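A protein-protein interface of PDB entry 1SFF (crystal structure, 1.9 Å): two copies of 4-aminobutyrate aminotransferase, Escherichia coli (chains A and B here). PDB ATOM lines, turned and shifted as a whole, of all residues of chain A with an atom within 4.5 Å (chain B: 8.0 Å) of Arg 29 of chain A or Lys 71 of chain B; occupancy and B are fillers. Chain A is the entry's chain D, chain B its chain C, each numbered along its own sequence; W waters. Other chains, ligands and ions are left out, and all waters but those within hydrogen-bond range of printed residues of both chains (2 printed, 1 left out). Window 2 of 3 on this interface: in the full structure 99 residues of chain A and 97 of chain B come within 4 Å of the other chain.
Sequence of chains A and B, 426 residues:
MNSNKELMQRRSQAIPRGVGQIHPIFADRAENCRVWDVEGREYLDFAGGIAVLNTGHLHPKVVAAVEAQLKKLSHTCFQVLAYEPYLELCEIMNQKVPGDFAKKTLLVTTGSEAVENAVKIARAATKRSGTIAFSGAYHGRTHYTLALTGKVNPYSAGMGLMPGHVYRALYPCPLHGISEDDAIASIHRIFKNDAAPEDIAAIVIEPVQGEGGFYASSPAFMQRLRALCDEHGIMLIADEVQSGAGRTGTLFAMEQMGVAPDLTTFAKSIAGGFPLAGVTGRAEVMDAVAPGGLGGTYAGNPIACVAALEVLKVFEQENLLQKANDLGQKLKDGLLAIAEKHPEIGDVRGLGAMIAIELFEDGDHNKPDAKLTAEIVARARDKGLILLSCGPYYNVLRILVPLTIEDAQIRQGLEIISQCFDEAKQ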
ATOM      1  N   ALA A  27      -8.593  36.315   5.488  1.00  0.00           N
ATOM      2  CA  ALA A  27      -8.857  35.015   6.088  1.00  0.00           C
ATOM      3  C   ALA A  27      -7.570  34.288   6.436  1.00  0.00           C
ATOM      4  O   ALA A  27      -6.606  34.334   5.689  1.00  0.00           O
ATOM      5  CB  ALA A  27      -9.684  34.132   5.093  1.00  0.00           C
ATOM      6  N   ASP A  28      -7.568  33.592   7.572  1.00  0.00           N
ATOM      7  CA  ASP A  28      -6.429  32.801   7.979  1.00  0.00           C
ATOM      8  C   ASP A  28      -6.786  31.288   7.907  1.00  0.00           C
ATOM      9  O   ASP A  28      -6.001  30.512   7.366  1.00  0.00           O
ATOM     10  CB  ASP A  28      -5.997  33.088   9.404  1.00  0.00           C
ATOM     11  CG  ASP A  28      -4.801  32.247   9.814  1.00  0.00           C
ATOM     12  OD1 ASP A  28      -3.724  32.370   9.176  1.00  0.00           O
ATOM     13  OD2 ASP A  28      -4.950  31.446  10.758  1.00  0.00           O
ATOM     14  N   ARG A  29      -7.916  30.887   8.497  1.00  0.00           N
ATOM     15  CA  ARG A  29      -8.343  29.461   8.467  1.00  0.00           C
ATOM     16  C   ARG A  29      -9.846  29.390   8.260  1.00  0.00           C
ATOM     17  O   ARG A  29     -10.541  30.386   8.450  1.00  0.00           O
ATOM     18  CB  ARG A  29      -7.998  28.710   9.789  1.00  0.00           C
ATOM     19  CG  ARG A  29      -6.533  28.725  10.162  1.00  0.00           C
ATOM     20  CD  ARG A  29      -6.315  28.183  11.581  1.00  0.00           C
ATOM     21  NE  ARG A  29      -6.652  26.766  11.679  1.00  0.00           N
ATOM     22  CZ  ARG A  29      -5.774  25.763  11.567  1.00  0.00           C
ATOM     23  NH1 ARG A  29      -4.469  26.019  11.357  1.00  0.00           N
ATOM     24  NH2 ARG A  29      -6.211  24.493  11.656  1.00  0.00           N
ATOM     25  N   ALA A  30     -10.355  28.200   7.910  1.00  0.00           N
ATOM     26  CA  ALA A  30     -11.766  28.056   7.679  1.00  0.00           C
ATOM     27  C   ALA A  30     -12.110  26.579   7.771  1.00  0.00           C
ATOM     28  O   ALA A  30     -11.262  25.738   7.528  1.00  0.00           O
ATOM     29  CB  ALA A  30     -12.119  28.590   6.295  1.00  0.00           C
ATOM     30  N   VAL A  35     -15.181  30.879   9.131  1.00  0.00           N
ATOM     31  CA  VAL A  35     -13.942  31.431   8.661  1.00  0.00           C
ATOM     32  C   VAL A  35     -13.340  32.287   9.812  1.00  0.00           C
ATOM     33  O   VAL A  35     -14.079  32.983  10.500  1.00  0.00           O
ATOM     34  CB  VAL A  35     -14.173  32.360   7.438  1.00  0.00           C
ATOM     35  CG1 VAL A  35     -12.867  32.958   7.002  1.00  0.00           C
ATOM     36  CG2 VAL A  35     -14.772  31.557   6.275  1.00  0.00           C
ATOM     37  N   TRP A  36     -12.026  32.222  10.022  1.00  0.00           N
ATOM     38  CA  TRP A  36     -11.403  33.056  11.064  1.00  0.00           C
ATOM     39  C   TRP A  36     -10.417  33.978  10.372  1.00  0.00           C
ATOM     40  O   TRP A  36      -9.610  33.515   9.566  1.00  0.00           O
ATOM     41  CB  TRP A  36     -10.660  32.185  12.089  1.00  0.00           C
ATOM     42  CG  TRP A  36     -11.579  31.361  12.915  1.00  0.00           C
ATOM     43  CD1 TRP A  36     -12.232  31.731  14.074  1.00  0.00           C
ATOM     44  CD2 TRP A  36     -12.059  30.037  12.586  1.00  0.00           C
ATOM     45  NE1 TRP A  36     -13.099  30.709  14.477  1.00  0.00           N
ATOM     46  CE2 TRP A  36     -13.007  29.666  13.584  1.00  0.00           C
ATOM     47  CE3 TRP A  36     -11.780  29.134  11.541  1.00  0.00           C
ATOM     48  CZ2 TRP A  36     -13.681  28.423  13.564  1.00  0.00           C
ATOM     49  CZ3 TRP A  36     -12.468  27.880  11.520  1.00  0.00           C
ATOM     50  CH2 TRP A  36     -13.398  27.551  12.525  1.00  0.00           C
ATOM     51  N   LEU A  58     -13.032  22.949   3.304  1.00  0.00           N
ATOM     52  CA  LEU A  58     -12.246  21.766   3.635  1.00  0.00           C
ATOM     53  C   LEU A  58     -13.035  20.558   4.165  1.00  0.00           C
ATOM     54  O   LEU A  58     -12.746  20.012   5.241  1.00  0.00           O
ATOM     55  CB  LEU A  58     -11.138  22.158   4.637  1.00  0.00           C
ATOM     56  CG  LEU A  58     -10.122  23.222   4.172  1.00  0.00           C
ATOM     57  CD1 LEU A  58      -9.265  23.607   5.379  1.00  0.00           C
ATOM     58  CD2 LEU A  58      -9.232  22.731   2.976  1.00  0.00           C
ATOM     59  N   ALA B  64       5.481  20.251   1.364  1.00  0.00           N
ATOM     60  CA  ALA B  64       5.300  20.554   2.778  1.00  0.00           C
ATOM     61  C   ALA B  64       4.495  21.860   2.960  1.00  0.00           C
ATOM     62  O   ALA B  64       3.597  21.928   3.806  1.00  0.00           O
ATOM     63  CB  ALA B  64       6.680  20.632   3.493  1.00  0.00           C
ATOM     64  N   ALA B  65       4.761  22.858   2.128  1.00  0.00           N
ATOM     65  CA  ALA B  65       4.046  24.140   2.243  1.00  0.00           C
ATOM     66  C   ALA B  65       2.579  23.962   1.899  1.00  0.00           C
ATOM     67  O   ALA B  65       1.699  24.533   2.556  1.00  0.00           O
ATOM     68  CB  ALA B  65       4.672  25.153   1.328  1.00  0.00           C
ATOM     69  N   VAL B  66       2.329  23.173   0.845  1.00  0.00           N
ATOM     70  CA  VAL B  66       0.982  22.862   0.410  1.00  0.00           C
ATOM     71  C   VAL B  66       0.244  22.130   1.523  1.00  0.00           C
ATOM     72  O   VAL B  66      -0.890  22.480   1.843  1.00  0.00           O
ATOM     73  CB  VAL B  66       1.006  21.979  -0.894  1.00  0.00           C
ATOM     74  CG1 VAL B  66      -0.373  21.371  -1.154  1.00  0.00           C
ATOM     75  CG2 VAL B  66       1.412  22.839  -2.099  1.00  0.00           C
ATOM     76  N   GLU B  67       0.873  21.114   2.119  1.00  0.00           N
ATOM     77  CA  GLU B  67       0.237  20.389   3.231  1.00  0.00           C
ATOM     78  C   GLU B  67      -0.119  21.306   4.416  1.00  0.00           C
ATOM     79  O   GLU B  67      -1.192  21.198   5.007  1.00  0.00           O
ATOM     80  CB  GLU B  67       1.143  19.235   3.676  1.00  0.00           C
ATOM     81  CG  GLU B  67       1.180  18.169   2.584  1.00  0.00           C
ATOM     82  CD  GLU B  67       1.905  16.901   2.937  1.00  0.00           C
ATOM     83  OE1 GLU B  67       2.851  16.943   3.740  1.00  0.00           O
ATOM     84  OE2 GLU B  67       1.533  15.854   2.360  1.00  0.00           O
ATOM     85  N   ALA B  68       0.764  22.232   4.743  1.00  0.00           N
ATOM     86  CA  ALA B  68       0.470  23.158   5.831  1.00  0.00           C
ATOM     87  C   ALA B  68      -0.744  24.034   5.476  1.00  0.00           C
ATOM     88  O   ALA B  68      -1.613  24.264   6.316  1.00  0.00           O
ATOM     89  CB  ALA B  68       1.692  24.036   6.097  1.00  0.00           C
ATOM     90  N   GLN B  69      -0.825  24.503   4.227  1.00  0.00           N
ATOM     91  CA  GLN B  69      -1.946  25.355   3.844  1.00  0.00           C
ATOM     92  C   GLN B  69      -3.250  24.582   3.771  1.00  0.00           C
ATOM     93  O   GLN B  69      -4.306  25.114   4.078  1.00  0.00           O
ATOM     94  CB  GLN B  69      -1.683  26.042   2.498  1.00  0.00           C
ATOM     95  CG  GLN B  69      -2.811  27.006   2.018  1.00  0.00           C
ATOM     96  CD  GLN B  69      -3.062  28.159   3.000  1.00  0.00           C
ATOM     97  OE1 GLN B  69      -2.118  28.696   3.577  1.00  0.00           O
ATOM     98  NE2 GLN B  69      -4.336  28.546   3.181  1.00  0.00           N
ATOM     99  N   LEU B  70      -3.178  23.316   3.382  1.00  0.00           N
ATOM    100  CA  LEU B  70      -4.388  22.493   3.288  1.00  0.00           C
ATOM    101  C   LEU B  70      -5.105  22.354   4.647  1.00  0.00           C
ATOM    102  O   LEU B  70      -6.310  22.062   4.722  1.00  0.00           O
ATOM    103  CB  LEU B  70      -3.994  21.123   2.746  1.00  0.00           C
ATOM    104  CG  LEU B  70      -5.105  20.122   2.438  1.00  0.00           C
ATOM    105  CD1 LEU B  70      -6.037  20.669   1.352  1.00  0.00           C
ATOM    106  CD2 LEU B  70      -4.437  18.808   1.966  1.00  0.00           C
ATOM    107  N   LYS B  71      -4.347  22.505   5.731  1.00  0.00           N
ATOM    108  CA  LYS B  71      -4.917  22.468   7.081  1.00  0.00           C
ATOM    109  C   LYS B  71      -5.657  23.786   7.407  1.00  0.00           C
ATOM    110  O   LYS B  71      -6.446  23.841   8.332  1.00  0.00           O
ATOM    111  CB  LYS B  71      -3.790  22.272   8.107  1.00  0.00           C
ATOM    112  CG  LYS B  71      -3.210  20.841   8.048  1.00  0.00           C
ATOM    113  CD  LYS B  71      -2.000  20.628   8.960  1.00  0.00           C
ATOM    114  CE  LYS B  71      -1.587  19.141   8.897  1.00  0.00           C
ATOM    115  NZ  LYS B  71      -0.208  18.872   9.425  1.00  0.00           N
ATOM    116  N   LYS B  72      -5.414  24.838   6.624  1.00  0.00           N
ATOM    117  CA  LYS B  72      -6.009  26.161   6.928  1.00  0.00           C
ATOM    118  C   LYS B  72      -7.224  26.463   6.092  1.00  0.00           C
ATOM    119  O   LYS B  72      -8.320  26.629   6.630  1.00  0.00           O
ATOM    120  CB  LYS B  72      -4.959  27.262   6.738  1.00  0.00           C
ATOM    121  CG  LYS B  72      -3.665  27.018   7.552  1.00  0.00           C
ATOM    122  CD  LYS B  72      -2.705  28.187   7.409  1.00  0.00           C
ATOM    123  CE  LYS B  72      -1.358  27.840   7.990  1.00  0.00           C
ATOM    124  NZ  LYS B  72      -0.409  28.997   7.796  1.00  0.00           N
ATOM    125  N   LEU B  73      -7.025  26.556   4.785  1.00  0.00           N
ATOM    126  CA  LEU B  73      -8.141  26.782   3.864  1.00  0.00           C
ATOM    127  C   LEU B  73      -7.683  26.587   2.430  1.00  0.00           C
ATOM    128  O   LEU B  73      -6.485  26.683   2.162  1.00  0.00           O
ATOM    129  CB  LEU B  73      -8.746  28.174   4.065  1.00  0.00           C
ATOM    130  CG  LEU B  73      -7.918  29.443   3.991  1.00  0.00           C
ATOM    131  CD1 LEU B  73      -7.639  29.811   2.563  1.00  0.00           C
ATOM    132  CD2 LEU B  73      -8.759  30.577   4.667  1.00  0.00           C
ATOM    133  N   SER B  74      -8.613  26.277   1.519  1.00  0.00           N
ATOM    134  CA  SER B  74      -8.216  26.085   0.110  1.00  0.00           C
ATOM    135  C   SER B  74      -8.819  27.142  -0.809  1.00  0.00           C
ATOM    136  O   SER B  74      -8.309  27.386  -1.878  1.00  0.00           O
ATOM    137  CB  SER B  74      -8.629  24.675  -0.388  1.00  0.00           C
ATOM    138  OG  SER B  74     -10.029  24.631  -0.642  1.00  0.00           O
ATOM    139  N   THR B  76     -11.275  31.072  -0.800  1.00  0.00           N
ATOM    140  CA  THR B  76     -12.266  32.020  -0.274  1.00  0.00           C
ATOM    141  C   THR B  76     -12.738  32.976  -1.394  1.00  0.00           C
ATOM    142  O   THR B  76     -13.772  33.598  -1.250  1.00  0.00           O
ATOM    143  CB  THR B  76     -11.707  32.968   0.826  1.00  0.00           C
ATOM    144  OG1 THR B  76     -10.589  33.682   0.299  1.00  0.00           O
ATOM    145  CG2 THR B  76     -11.322  32.203   2.069  1.00  0.00           C
ATOM    146  N   LEU B  81     -12.847  37.673   0.193  1.00  0.00           N
ATOM    147  CA  LEU B  81     -12.149  37.659   1.482  1.00  0.00           C
ATOM    148  C   LEU B  81     -10.723  37.402   1.061  1.00  0.00           C
ATOM    149  O   LEU B  81     -10.438  36.365   0.458  1.00  0.00           O
ATOM    150  CB  LEU B  81     -12.613  36.503   2.379  1.00  0.00           C
ATOM    151  CG  LEU B  81     -13.370  36.773   3.669  1.00  0.00           C
ATOM    152  CD1 LEU B  81     -14.593  37.570   3.407  1.00  0.00           C
ATOM    153  CD2 LEU B  81     -13.758  35.431   4.287  1.00  0.00           C
ATOM    154  N   TYR B  83      -6.399  36.940   1.485  1.00  0.00           N
ATOM    155  CA  TYR B  83      -5.558  36.052   2.300  1.00  0.00           C
ATOM    156  C   TYR B  83      -4.119  36.432   2.047  1.00  0.00           C
ATOM    157  O   TYR B  83      -3.775  36.907   0.969  1.00  0.00           O
ATOM    158  CB  TYR B  83      -5.812  34.541   2.029  1.00  0.00           C
ATOM    159  CG  TYR B  83      -6.130  34.226   0.581  1.00  0.00           C
ATOM    160  CD1 TYR B  83      -5.123  33.955  -0.351  1.00  0.00           C
ATOM    161  CD2 TYR B  83      -7.435  34.241   0.150  1.00  0.00           C
ATOM    162  CE1 TYR B  83      -5.455  33.708  -1.723  1.00  0.00           C
ATOM    163  CE2 TYR B  83      -7.772  34.000  -1.187  1.00  0.00           C
ATOM    164  CZ  TYR B  83      -6.792  33.737  -2.111  1.00  0.00           C
ATOM    165  OH  TYR B  83      -7.187  33.472  -3.425  1.00  0.00           O
ATOM    166  N   ILE B 303      -3.652  27.472  -2.051  1.00  0.00           N
ATOM    167  CA  ILE B 303      -2.671  26.401  -2.071  1.00  0.00           C
ATOM    168  C   ILE B 303      -1.593  26.597  -3.121  1.00  0.00           C
ATOM    169  O   ILE B 303      -0.418  26.332  -2.876  1.00  0.00           O
ATOM    170  CB  ILE B 303      -3.398  25.064  -2.229  1.00  0.00           C
ATOM    171  CG1 ILE B 303      -4.210  24.815  -0.946  1.00  0.00           C
ATOM    172  CG2 ILE B 303      -2.405  23.953  -2.456  1.00  0.00           C
ATOM    173  CD1 ILE B 303      -5.051  23.598  -0.975  1.00  0.00           C
HETATM  174  O   HOH W   1     -12.277  23.782   0.520  1.00  0.00           O
HETATM  175  O   HOH W   2      -1.249  31.104   8.817  1.00  0.00           O
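Printed residues of chain A that touch a printed residue of chain B: Ala 27, Asp 28, Arg 29, Ala 30, Val 35 and Leu 58. Along chain A the printed residues that touch a printed residue of chain B span positions 27 to 58. Hydrophobic or aromatic side chains of chain B within 4 Å of the printed part of chain A: Leu 73, Leu 81 and Tyr 83. Among the printed residues, 14 pairs touch across the chains. Among the printed residues, no Asp or Glu carboxylate lies within 4 Å of a Lys or Arg side-chain nitrogen of the other chain.
O of Lys 71 of chain B lies within hydrogen-bond range of NH2 of Arg 29 of chain A, at 3.4 Å. The backbone carbonyl oxygen (O) of Lys 72 of chain B lies within hydrogen-bond range of the backbone NH (N) of Ala 30 of chain A (2.9 Å).
Water W2 bridges the side-chain amino group of Lys 72 of chain B (2.5 Å) and the side-chain carboxylate of Asp 28 of chain A (2.8 Å). Water W1 bridges the side-chain hydroxyl (OG) of Ser 74 of chain B (2.7 Å) and the backbone NH (N) of Leu 58 of chain A (3.0 Å).
The side-chain amide nitrogen of Gln 69 of chain B is in hydrogen-bond range of the backbone carbonyl oxygen of Leu 73 of chain B (3.0 Å). The side-chain hydroxyl (OG1) of Thr 76 of chain B is in hydrogen-bond range of the backbone carbonyl oxygen (O) of Leu 81 of chain B (2.7 Å). O of Trp 36 of chain A lies within hydrogen-bond range of N of Asp 28 of chain A (2.9 Å). O of Arg 29 of chain A is in hydrogen-bond range of N of Trp 36 of chain A.
Among the printed residues, pairs that only touch across the chains: Ala 27 of chain A with Leu 73 of chain B, Ala 27 of chain A with Thr 76 of chain B, Ala 27 of chain A with Tyr 83 of chain B, Asp 28 of chain A with Lys 72 of chain B, Asp 28 of chain A with Leu 73 of chain B, Arg 29 of chain A with Lys 72 of chain B, Arg 29 of chain A with Leu 73 of chain B, Val 35 of chain A with Leu 81 of chain B, Leu 58 of chain A with Leu 70 of chain B, Leu 58 of chain A with Lys 72 of chain B, Leu 58 of chain A with Leu 73 of chain B and Leu 58 of chain A with Ser 74 of chain B.
Arg 29 of chain A touches three residues of chain B. Of chain A, only Arg 29 (3.4 Å) comes within 4 Å of Lys 71 of chain B. Of the printed residues of chain B, Ala 27 of chain A touches Leu 73, Thr 76 and Tyr 83. Of the printed residues of chain B, Asp 28 of chain A touches Lys 72 (3.5 Å) and Leu 73 (3.9 Å). Gln 69 of chain B touches none of the printed residues of chain A. The nearest residue of chain B that does not touch Arg 29 of chain A is Ala 68 of chain B (6.1 Å). The nearest printed residue of chain A that does not touch Tyr 83 of chain B is Asp 28 of chain A (5.9 Å).
No position is printed for both chains.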
